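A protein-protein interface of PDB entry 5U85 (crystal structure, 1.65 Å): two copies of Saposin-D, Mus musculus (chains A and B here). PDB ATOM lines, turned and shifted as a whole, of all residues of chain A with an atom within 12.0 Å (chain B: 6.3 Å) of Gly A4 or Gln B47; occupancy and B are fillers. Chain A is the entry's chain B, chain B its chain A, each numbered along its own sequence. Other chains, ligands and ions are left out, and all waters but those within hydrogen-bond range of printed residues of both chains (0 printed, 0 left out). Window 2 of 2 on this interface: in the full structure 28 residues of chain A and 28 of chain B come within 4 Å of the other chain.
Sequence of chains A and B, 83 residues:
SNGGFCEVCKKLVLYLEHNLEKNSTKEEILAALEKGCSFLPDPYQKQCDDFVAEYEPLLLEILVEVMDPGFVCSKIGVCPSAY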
ATOM      1  N   GLY A   4      18.085  28.190  20.550  1.00  0.00           N
ATOM      2  CA  GLY A   4      17.161  27.139  20.165  1.00  0.00           C
ATOM      3  C   GLY A   4      17.643  26.288  19.002  1.00  0.00           C
ATOM      4  O   GLY A   4      17.753  25.064  19.118  1.00  0.00           O
ATOM      5  N   PHE A   5      17.923  26.944  17.875  1.00  0.00           N
ATOM      6  CA  PHE A   5      18.377  26.280  16.658  1.00  0.00           C
ATOM      7  C   PHE A   5      19.890  26.148  16.578  1.00  0.00           C
ATOM      8  O   PHE A   5      20.398  25.609  15.590  1.00  0.00           O
ATOM      9  CB  PHE A   5      17.902  27.049  15.413  1.00  0.00           C
ATOM     10  CG  PHE A   5      16.425  26.918  15.114  1.00  0.00           C
ATOM     11  CD1 PHE A   5      15.722  25.755  15.396  1.00  0.00           C
ATOM     12  CD2 PHE A   5      15.743  27.976  14.535  1.00  0.00           C
ATOM     13  CE1 PHE A   5      14.365  25.654  15.106  1.00  0.00           C
ATOM     14  CE2 PHE A   5      14.394  27.887  14.245  1.00  0.00           C
ATOM     15  CZ  PHE A   5      13.700  26.725  14.530  1.00  0.00           C
ATOM     16  N   CYS A   6      20.629  26.651  17.566  1.00  0.00           N
ATOM     17  CA  CYS A   6      22.079  26.710  17.421  1.00  0.00           C
ATOM     18  C   CYS A   6      22.673  25.324  17.210  1.00  0.00           C
ATOM     19  O   CYS A   6      23.489  25.112  16.305  1.00  0.00           O
ATOM     20  CB  CYS A   6      22.711  27.365  18.648  1.00  0.00           C
ATOM     21  SG  CYS A   6      24.518  27.383  18.583  1.00  0.00           S
ATOM     22  N   GLU A   7      22.268  24.359  18.035  1.00  0.00           N
ATOM     23  CA  GLU A   7      22.900  23.044  17.982  1.00  0.00           C
ATOM     24  C   GLU A   7      22.467  22.265  16.740  1.00  0.00           C
ATOM     25  O   GLU A   7      23.261  21.499  16.185  1.00  0.00           O
ATOM     26  CB  GLU A   7      22.625  22.267  19.274  1.00  0.00           C
ATOM     27  CG  GLU A   7      23.322  22.912  20.480  1.00  0.00           C
ATOM     28  CD  GLU A   7      24.839  22.890  20.366  1.00  0.00           C
ATOM     29  OE1 GLU A   7      25.388  21.859  19.923  1.00  0.00           O
ATOM     30  OE2 GLU A   7      25.479  23.911  20.706  1.00  0.00           O
ATOM     31  N   VAL A   8      21.224  22.442  16.276  1.00  0.00           N
ATOM     32  CA  VAL A   8      20.817  21.697  15.085  1.00  0.00           C
ATOM     33  C   VAL A   8      21.452  22.295  13.835  1.00  0.00           C
ATOM     34  O   VAL A   8      21.775  21.572  12.882  1.00  0.00           O
ATOM     35  CB  VAL A   8      19.283  21.640  14.967  1.00  0.00           C
ATOM     36  CG1 VAL A   8      18.709  23.011  14.578  1.00  0.00           C
ATOM     37  CG2 VAL A   8      18.881  20.566  13.947  1.00  0.00           C
ATOM     38  N   CYS A   9      21.648  23.614  13.812  1.00  0.00           N
ATOM     39  CA  CYS A   9      22.340  24.239  12.690  1.00  0.00           C
ATOM     40  C   CYS A   9      23.751  23.684  12.544  1.00  0.00           C
ATOM     41  O   CYS A   9      24.176  23.311  11.444  1.00  0.00           O
ATOM     42  CB  CYS A   9      22.379  25.760  12.868  1.00  0.00           C
ATOM     43  SG  CYS A   9      23.271  26.624  11.545  1.00  0.00           S
ATOM     44  N   LYS A  10      24.498  23.620  13.649  1.00  0.00           N
ATOM     45  CA  LYS A  10      25.866  23.117  13.588  1.00  0.00           C
ATOM     46  C   LYS A  10      25.898  21.646  13.191  1.00  0.00           C
ATOM     47  O   LYS A  10      26.758  21.228  12.406  1.00  0.00           O
ATOM     48  CB  LYS A  10      26.557  23.338  14.934  1.00  0.00           C
ATOM     49  CG  LYS A  10      26.861  24.803  15.220  1.00  0.00           C
ATOM     50  CD  LYS A  10      27.724  24.990  16.460  1.00  0.00           C
ATOM     51  CE  LYS A  10      26.975  24.632  17.734  1.00  0.00           C
ATOM     52  NZ  LYS A  10      27.734  25.035  18.952  1.00  0.00           N
ATOM     53  N   LYS A  11      24.966  20.845  13.715  1.00  0.00           N
ATOM     54  CA  LYS A  11      24.895  19.442  13.320  1.00  0.00           C
ATOM     55  C   LYS A  11      24.604  19.304  11.832  1.00  0.00           C
ATOM     56  O   LYS A  11      25.153  18.420  11.164  1.00  0.00           O
ATOM     57  CB  LYS A  11      23.824  18.717  14.136  1.00  0.00           C
ATOM     58  CG  LYS A  11      24.187  18.492  15.594  1.00  0.00           C
ATOM     59  CD  LYS A  11      22.973  18.048  16.401  1.00  0.00           C
ATOM     60  CE  LYS A  11      23.203  16.710  17.083  1.00  0.00           C
ATOM     61  NZ  LYS A  11      23.418  15.610  16.103  1.00  0.00           N
ATOM     62  N   LEU A  12      23.731  20.162  11.292  1.00  0.00           N
ATOM     63  CA  LEU A  12      23.385  20.068   9.875  1.00  0.00           C
ATOM     64  C   LEU A  12      24.567  20.434   8.988  1.00  0.00           C
ATOM     65  O   LEU A  12      24.800  19.783   7.962  1.00  0.00           O
ATOM     66  CB  LEU A  12      22.191  20.966   9.555  1.00  0.00           C
ATOM     67  CG  LEU A  12      20.808  20.372   9.817  1.00  0.00           C
ATOM     68  CD1 LEU A  12      19.753  21.459   9.703  1.00  0.00           C
ATOM     69  CD2 LEU A  12      20.525  19.234   8.844  1.00  0.00           C
ATOM     70  N   CYS A  73      26.766  29.240  11.452  1.00  0.00           N
ATOM     71  CA  CYS A  73      25.537  29.309  12.229  1.00  0.00           C
ATOM     72  C   CYS A  73      25.451  30.584  13.057  1.00  0.00           C
ATOM     73  O   CYS A  73      24.344  31.052  13.349  1.00  0.00           O
ATOM     74  CB  CYS A  73      25.429  28.067  13.110  1.00  0.00           C
ATOM     75  SG  CYS A  73      25.218  26.563  12.117  1.00  0.00           S
ATOM     76  N   SER A  74      26.590  31.167  13.438  1.00  0.00           N
ATOM     77  CA  SER A  74      26.556  32.496  14.035  1.00  0.00           C
ATOM     78  C   SER A  74      26.273  33.561  12.983  1.00  0.00           C
ATOM     79  O   SER A  74      25.622  34.569  13.280  1.00  0.00           O
ATOM     80  CB  SER A  74      27.874  32.797  14.752  1.00  0.00           C
ATOM     81  OG  SER A  74      28.914  33.069  13.828  1.00  0.00           O
ATOM     82  N   ILE A  76      24.252  33.421  10.422  1.00  0.00           N
ATOM     83  CA  ILE A  76      22.804  33.541  10.251  1.00  0.00           C
ATOM     84  C   ILE A  76      22.092  33.851  11.557  1.00  0.00           C
ATOM     85  O   ILE A  76      20.862  33.981  11.564  1.00  0.00           O
ATOM     86  CB  ILE A  76      22.187  32.275   9.621  1.00  0.00           C
ATOM     87  CG1 ILE A  76      22.333  31.057  10.540  1.00  0.00           C
ATOM     88  CG2 ILE A  76      22.827  31.995   8.266  1.00  0.00           C
ATOM     89  CD1 ILE A  76      21.438  29.897  10.142  1.00  0.00           C
ATOM     90  N   GLY A  77      22.823  33.958  12.664  1.00  0.00           N
ATOM     91  CA  GLY A  77      22.269  34.492  13.891  1.00  0.00           C
ATOM     92  C   GLY A  77      21.570  33.507  14.800  1.00  0.00           C
ATOM     93  O   GLY A  77      20.811  33.937  15.675  1.00  0.00           O
ATOM     94  N   VAL A  78      21.797  32.200  14.637  1.00  0.00           N
ATOM     95  CA  VAL A  78      21.196  31.216  15.532  1.00  0.00           C
ATOM     96  C   VAL A  78      22.167  30.724  16.599  1.00  0.00           C
ATOM     97  O   VAL A  78      21.733  30.047  17.543  1.00  0.00           O
ATOM     98  CB  VAL A  78      20.621  30.014  14.749  1.00  0.00           C
ATOM     99  CG1 VAL A  78      19.555  30.485  13.766  1.00  0.00           C
ATOM    100  CG2 VAL A  78      21.717  29.250  14.023  1.00  0.00           C
ATOM    101  N   CYS A  79      23.454  31.049  16.488  1.00  0.00           N
ATOM    102  CA  CYS A  79      24.466  30.697  17.470  1.00  0.00           C
ATOM    103  C   CYS A  79      25.212  31.946  17.912  1.00  0.00           C
ATOM    104  O   CYS A  79      25.270  32.931  17.169  1.00  0.00           O
ATOM    105  CB  CYS A  79      25.487  29.702  16.899  1.00  0.00           C
ATOM    106  SG  CYS A  79      24.935  28.006  16.699  1.00  0.00           S
ATOM    107  N   PRO A  80      25.805  31.935  19.117  1.00  0.00           N
ATOM    108  CA  PRO A  80      26.749  33.011  19.435  1.00  0.00           C
ATOM    109  C   PRO A  80      27.982  32.957  18.534  1.00  0.00           C
ATOM    110  O   PRO A  80      28.642  33.976  18.340  1.00  0.00           O
ATOM    111  CB  PRO A  80      27.126  32.741  20.897  1.00  0.00           C
ATOM    112  CG  PRO A  80      26.045  31.872  21.432  1.00  0.00           C
ATOM    113  CD  PRO A  80      25.558  31.057  20.274  1.00  0.00           C
ATOM    114  N   CYS B  37      17.848  16.064   8.508  1.00  0.00           N
ATOM    115  CA  CYS B  37      16.838  16.118   9.560  1.00  0.00           C
ATOM    116  C   CYS B  37      16.132  14.780   9.732  1.00  0.00           C
ATOM    117  O   CYS B  37      15.708  14.442  10.843  1.00  0.00           O
ATOM    118  CB  CYS B  37      15.806  17.205   9.251  1.00  0.00           C
ATOM    119  SG  CYS B  37      16.435  18.901   9.218  1.00  0.00           S
ATOM    120  N   PRO B  43      10.701  14.559  18.945  1.00  0.00           N
ATOM    121  CA  PRO B  43      10.202  15.704  18.181  1.00  0.00           C
ATOM    122  C   PRO B  43      11.306  16.463  17.447  1.00  0.00           C
ATOM    123  O   PRO B  43      11.054  17.542  16.908  1.00  0.00           O
ATOM    124  CB  PRO B  43       9.587  16.580  19.265  1.00  0.00           C
ATOM    125  CG  PRO B  43      10.501  16.361  20.434  1.00  0.00           C
ATOM    126  CD  PRO B  43      10.949  14.918  20.352  1.00  0.00           C
ATOM    127  N   TYR B  44      12.514  15.899  17.428  1.00  0.00           N
ATOM    128  CA  TYR B  44      13.669  16.645  16.943  1.00  0.00           C
ATOM    129  C   TYR B  44      13.692  16.769  15.425  1.00  0.00           C
ATOM    130  O   TYR B  44      14.229  17.755  14.905  1.00  0.00           O
ATOM    131  CB  TYR B  44      14.955  15.989  17.442  1.00  0.00           C
ATOM    132  CG  TYR B  44      14.996  15.844  18.946  1.00  0.00           C
ATOM    133  CD1 TYR B  44      15.154  16.953  19.766  1.00  0.00           C
ATOM    134  CD2 TYR B  44      14.869  14.599  19.546  1.00  0.00           C
ATOM    135  CE1 TYR B  44      15.187  16.825  21.142  1.00  0.00           C
ATOM    136  CE2 TYR B  44      14.902  14.460  20.919  1.00  0.00           C
ATOM    137  CZ  TYR B  44      15.062  15.576  21.712  1.00  0.00           C
ATOM    138  OH  TYR B  44      15.095  15.442  23.081  1.00  0.00           O
ATOM    139  N   GLN B  45      13.128  15.804  14.693  1.00  0.00           N
ATOM    140  CA  GLN B  45      13.054  15.954  13.244  1.00  0.00           C
ATOM    141  C   GLN B  45      12.246  17.189  12.870  1.00  0.00           C
ATOM    142  O   GLN B  45      12.641  17.952  11.981  1.00  0.00           O
ATOM    143  CB  GLN B  45      12.449  14.708  12.591  1.00  0.00           C
ATOM    144  CG  GLN B  45      12.315  14.846  11.070  1.00  0.00           C
ATOM    145  CD  GLN B  45      11.806  13.595  10.383  1.00  0.00           C
ATOM    146  OE1 GLN B  45      11.382  12.638  11.031  1.00  0.00           O
ATOM    147  NE2 GLN B  45      11.846  13.599   9.053  1.00  0.00           N
ATOM    148  N   LYS B  46      11.109  17.404  13.540  1.00  0.00           N
ATOM    149  CA  LYS B  46      10.278  18.562  13.229  1.00  0.00           C
ATOM    150  C   LYS B  46      11.009  19.864  13.534  1.00  0.00           C
ATOM    151  O   LYS B  46      10.922  20.824  12.760  1.00  0.00           O
ATOM    152  CB  LYS B  46       8.965  18.496  14.008  1.00  0.00           C
ATOM    153  CG  LYS B  46       7.996  19.623  13.666  1.00  0.00           C
ATOM    154  CD  LYS B  46       7.072  19.948  14.826  1.00  0.00           C
ATOM    155  CE  LYS B  46       6.214  21.165  14.518  1.00  0.00           C
ATOM    156  NZ  LYS B  46       6.985  22.438  14.629  1.00  0.00           N
ATOM    157  N   GLN B  47      11.717  19.924  14.665  1.00  0.00           N
ATOM    158  CA  GLN B  47      12.491  21.122  14.980  1.00  0.00           C
ATOM    159  C   GLN B  47      13.522  21.394  13.897  1.00  0.00           C
ATOM    160  O   GLN B  47      13.691  22.538  13.456  1.00  0.00           O
ATOM    161  CB  GLN B  47      13.177  20.973  16.340  1.00  0.00           C
ATOM    162  CG  GLN B  47      14.138  22.115  16.684  1.00  0.00           C
ATOM    163  CD  GLN B  47      15.019  21.809  17.878  1.00  0.00           C
ATOM    164  OE1 GLN B  47      15.491  20.685  18.047  1.00  0.00           O
ATOM    165  NE2 GLN B  47      15.251  22.815  18.711  1.00  0.00           N
ATOM    166  N   CYS B  48      14.229  20.349  13.463  1.00  0.00           N
ATOM    167  CA  CYS B  48      15.204  20.492  12.387  1.00  0.00           C
ATOM    168  C   CYS B  48      14.532  20.943  11.097  1.00  0.00           C
ATOM    169  O   CYS B  48      15.028  21.847  10.412  1.00  0.00           O
ATOM    170  CB  CYS B  48      15.934  19.161  12.196  1.00  0.00           C
ATOM    171  SG  CYS B  48      17.314  19.149  11.035  1.00  0.00           S
ATOM    172  N   ASP B  49      13.394  20.333  10.751  1.00  0.00           N
ATOM    173  CA  ASP B  49      12.660  20.757   9.562  1.00  0.00           C
ATOM    174  C   ASP B  49      12.252  22.220   9.662  1.00  0.00           C
ATOM    175  O   ASP B  49      12.301  22.955   8.668  1.00  0.00           O
ATOM    176  CB  ASP B  49      11.426  19.877   9.359  1.00  0.00           C
ATOM    177  CG  ASP B  49      11.778  18.471   8.914  1.00  0.00           C
ATOM    178  OD1 ASP B  49      12.867  18.283   8.331  1.00  0.00           O
ATOM    179  OD2 ASP B  49      10.961  17.555   9.140  1.00  0.00           O
ATOM    180  N   ASP B  50      11.842  22.660  10.854  1.00  0.00           N
ATOM    181  CA  ASP B  50      11.461  24.057  11.036  1.00  0.00           C
ATOM    182  C   ASP B  50      12.645  24.984  10.798  1.00  0.00           C
ATOM    183  O   ASP B  50      12.504  26.034  10.160  1.00  0.00           O
ATOM    184  CB  ASP B  50      10.898  24.272  12.438  1.00  0.00           C
ATOM    185  CG  ASP B  50       9.538  23.635  12.623  1.00  0.00           C
ATOM    186  OD1 ASP B  50       8.894  23.295  11.608  1.00  0.00           O
ATOM    187  OD2 ASP B  50       9.110  23.481  13.785  1.00  0.00           O
ATOM    188  N   PHE B  51      13.818  24.621  11.315  1.00  0.00           N
ATOM    189  CA  PHE B  51      15.007  25.426  11.071  1.00  0.00           C
ATOM    190  C   PHE B  51      15.292  25.537   9.579  1.00  0.00           C
ATOM    191  O   PHE B  51      15.540  26.631   9.059  1.00  0.00           O
ATOM    192  CB  PHE B  51      16.214  24.829  11.788  1.00  0.00           C
ATOM    193  CG  PHE B  51      17.515  25.404  11.326  1.00  0.00           C
ATOM    194  CD1 PHE B  51      17.898  26.674  11.719  1.00  0.00           C
ATOM    195  CD2 PHE B  51      18.341  24.691  10.474  1.00  0.00           C
ATOM    196  CE1 PHE B  51      19.088  27.219  11.284  1.00  0.00           C
ATOM    197  CE2 PHE B  51      19.534  25.229  10.036  1.00  0.00           C
ATOM    198  CZ  PHE B  51      19.909  26.496  10.441  1.00  0.00           C
ATOM    199  N   VAL B  52      15.268  24.403   8.876  1.00  0.00           N
ATOM    200  CA  VAL B  52      15.575  24.401   7.449  1.00  0.00           C
ATOM    201  C   VAL B  52      14.575  25.264   6.691  1.00  0.00           C
ATOM    202  O   VAL B  52      14.947  26.027   5.789  1.00  0.00           O
ATOM    203  CB  VAL B  52      15.604  22.954   6.921  1.00  0.00           C
ATOM    204  CG1 VAL B  52      15.662  22.922   5.401  1.00  0.00           C
ATOM    205  CG2 VAL B  52      16.795  22.207   7.505  1.00  0.00           C
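Of the 16 printed residues of chain A, 6 touch a printed residue of chain B. Hydrophobic or aromatic side chains of chain A that line the printed part of chain B: Phe A5, Val A8, Leu A12 and Ile A76. Of the 11 printed residues of chain B, 4 touch a printed residue of chain A. Printed residues of chain B that touch a printed residue of chain A: Gln B47, Cys B48, Phe B51 and Val B52. Hydrophobic or aromatic side chains of chain B within 4 Å of the printed part of chain A: Phe B51 and Val B52. Among the printed residues, 9 pairs touch across the chains. Among the printed residues, no Asp or Glu carboxylate lies within 4 Å of a Lys or Arg side-chain nitrogen of the other chain.
The side-chain amide nitrogen (NE2) of Gln B47 is in hydrogen-bond range of the backbone carbonyl oxygen (O) of Gly A4, 3.4 Å away.
Of chain B, only Gln B47 (3.4 Å) comes within 4 Å of Gly A4. Of the printed residues of chain A, Gln B47 touches Gly A4 (3.4 Å) and Phe A5 (3.6 Å). Cys B48 touches just these residues of chain A: Val A8 and Leu A12. Printed residues of chain B within 4 Å of Val A8: Cys B48 (3.6 Å). Of the printed residues of chain B, Cys A9 touches Phe B51. The nearest printed residue of chain B that does not touch Gly A4 is Phe B51 (7.3 Å).
No position is printed for both chains.
Among the printed residues, merely in contact across the chains: Phe A5 with Gln B47 (3.6 Å), Phe A5 with Phe B51 (3.7 Å), Val A8 with Cys B48 (3.6 Å), Cys A9 with Phe B51 (3.5 Å), Leu A12 with Cys B48 (3.6 Å), Leu A12 with Phe B51 (3.6 Å), Leu A12 with Val B52 (3.8 Å) and Ile A76 with Phe B51 (3.7 Å).
The side-chain sulfur (SG) of Cys B37 forms a disulfide with the side-chain sulfur (SG) of Cys B48 (2.0 Å). The side-chain sulfur (SG) of Cys A9 forms a disulfide with the side-chain sulfur (SG) of Cys A73 (2.0 Å). The side-chain sulfur of Cys A6 forms a disulfide with the side-chain sulfur of Cys A79 (2.0 Å).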
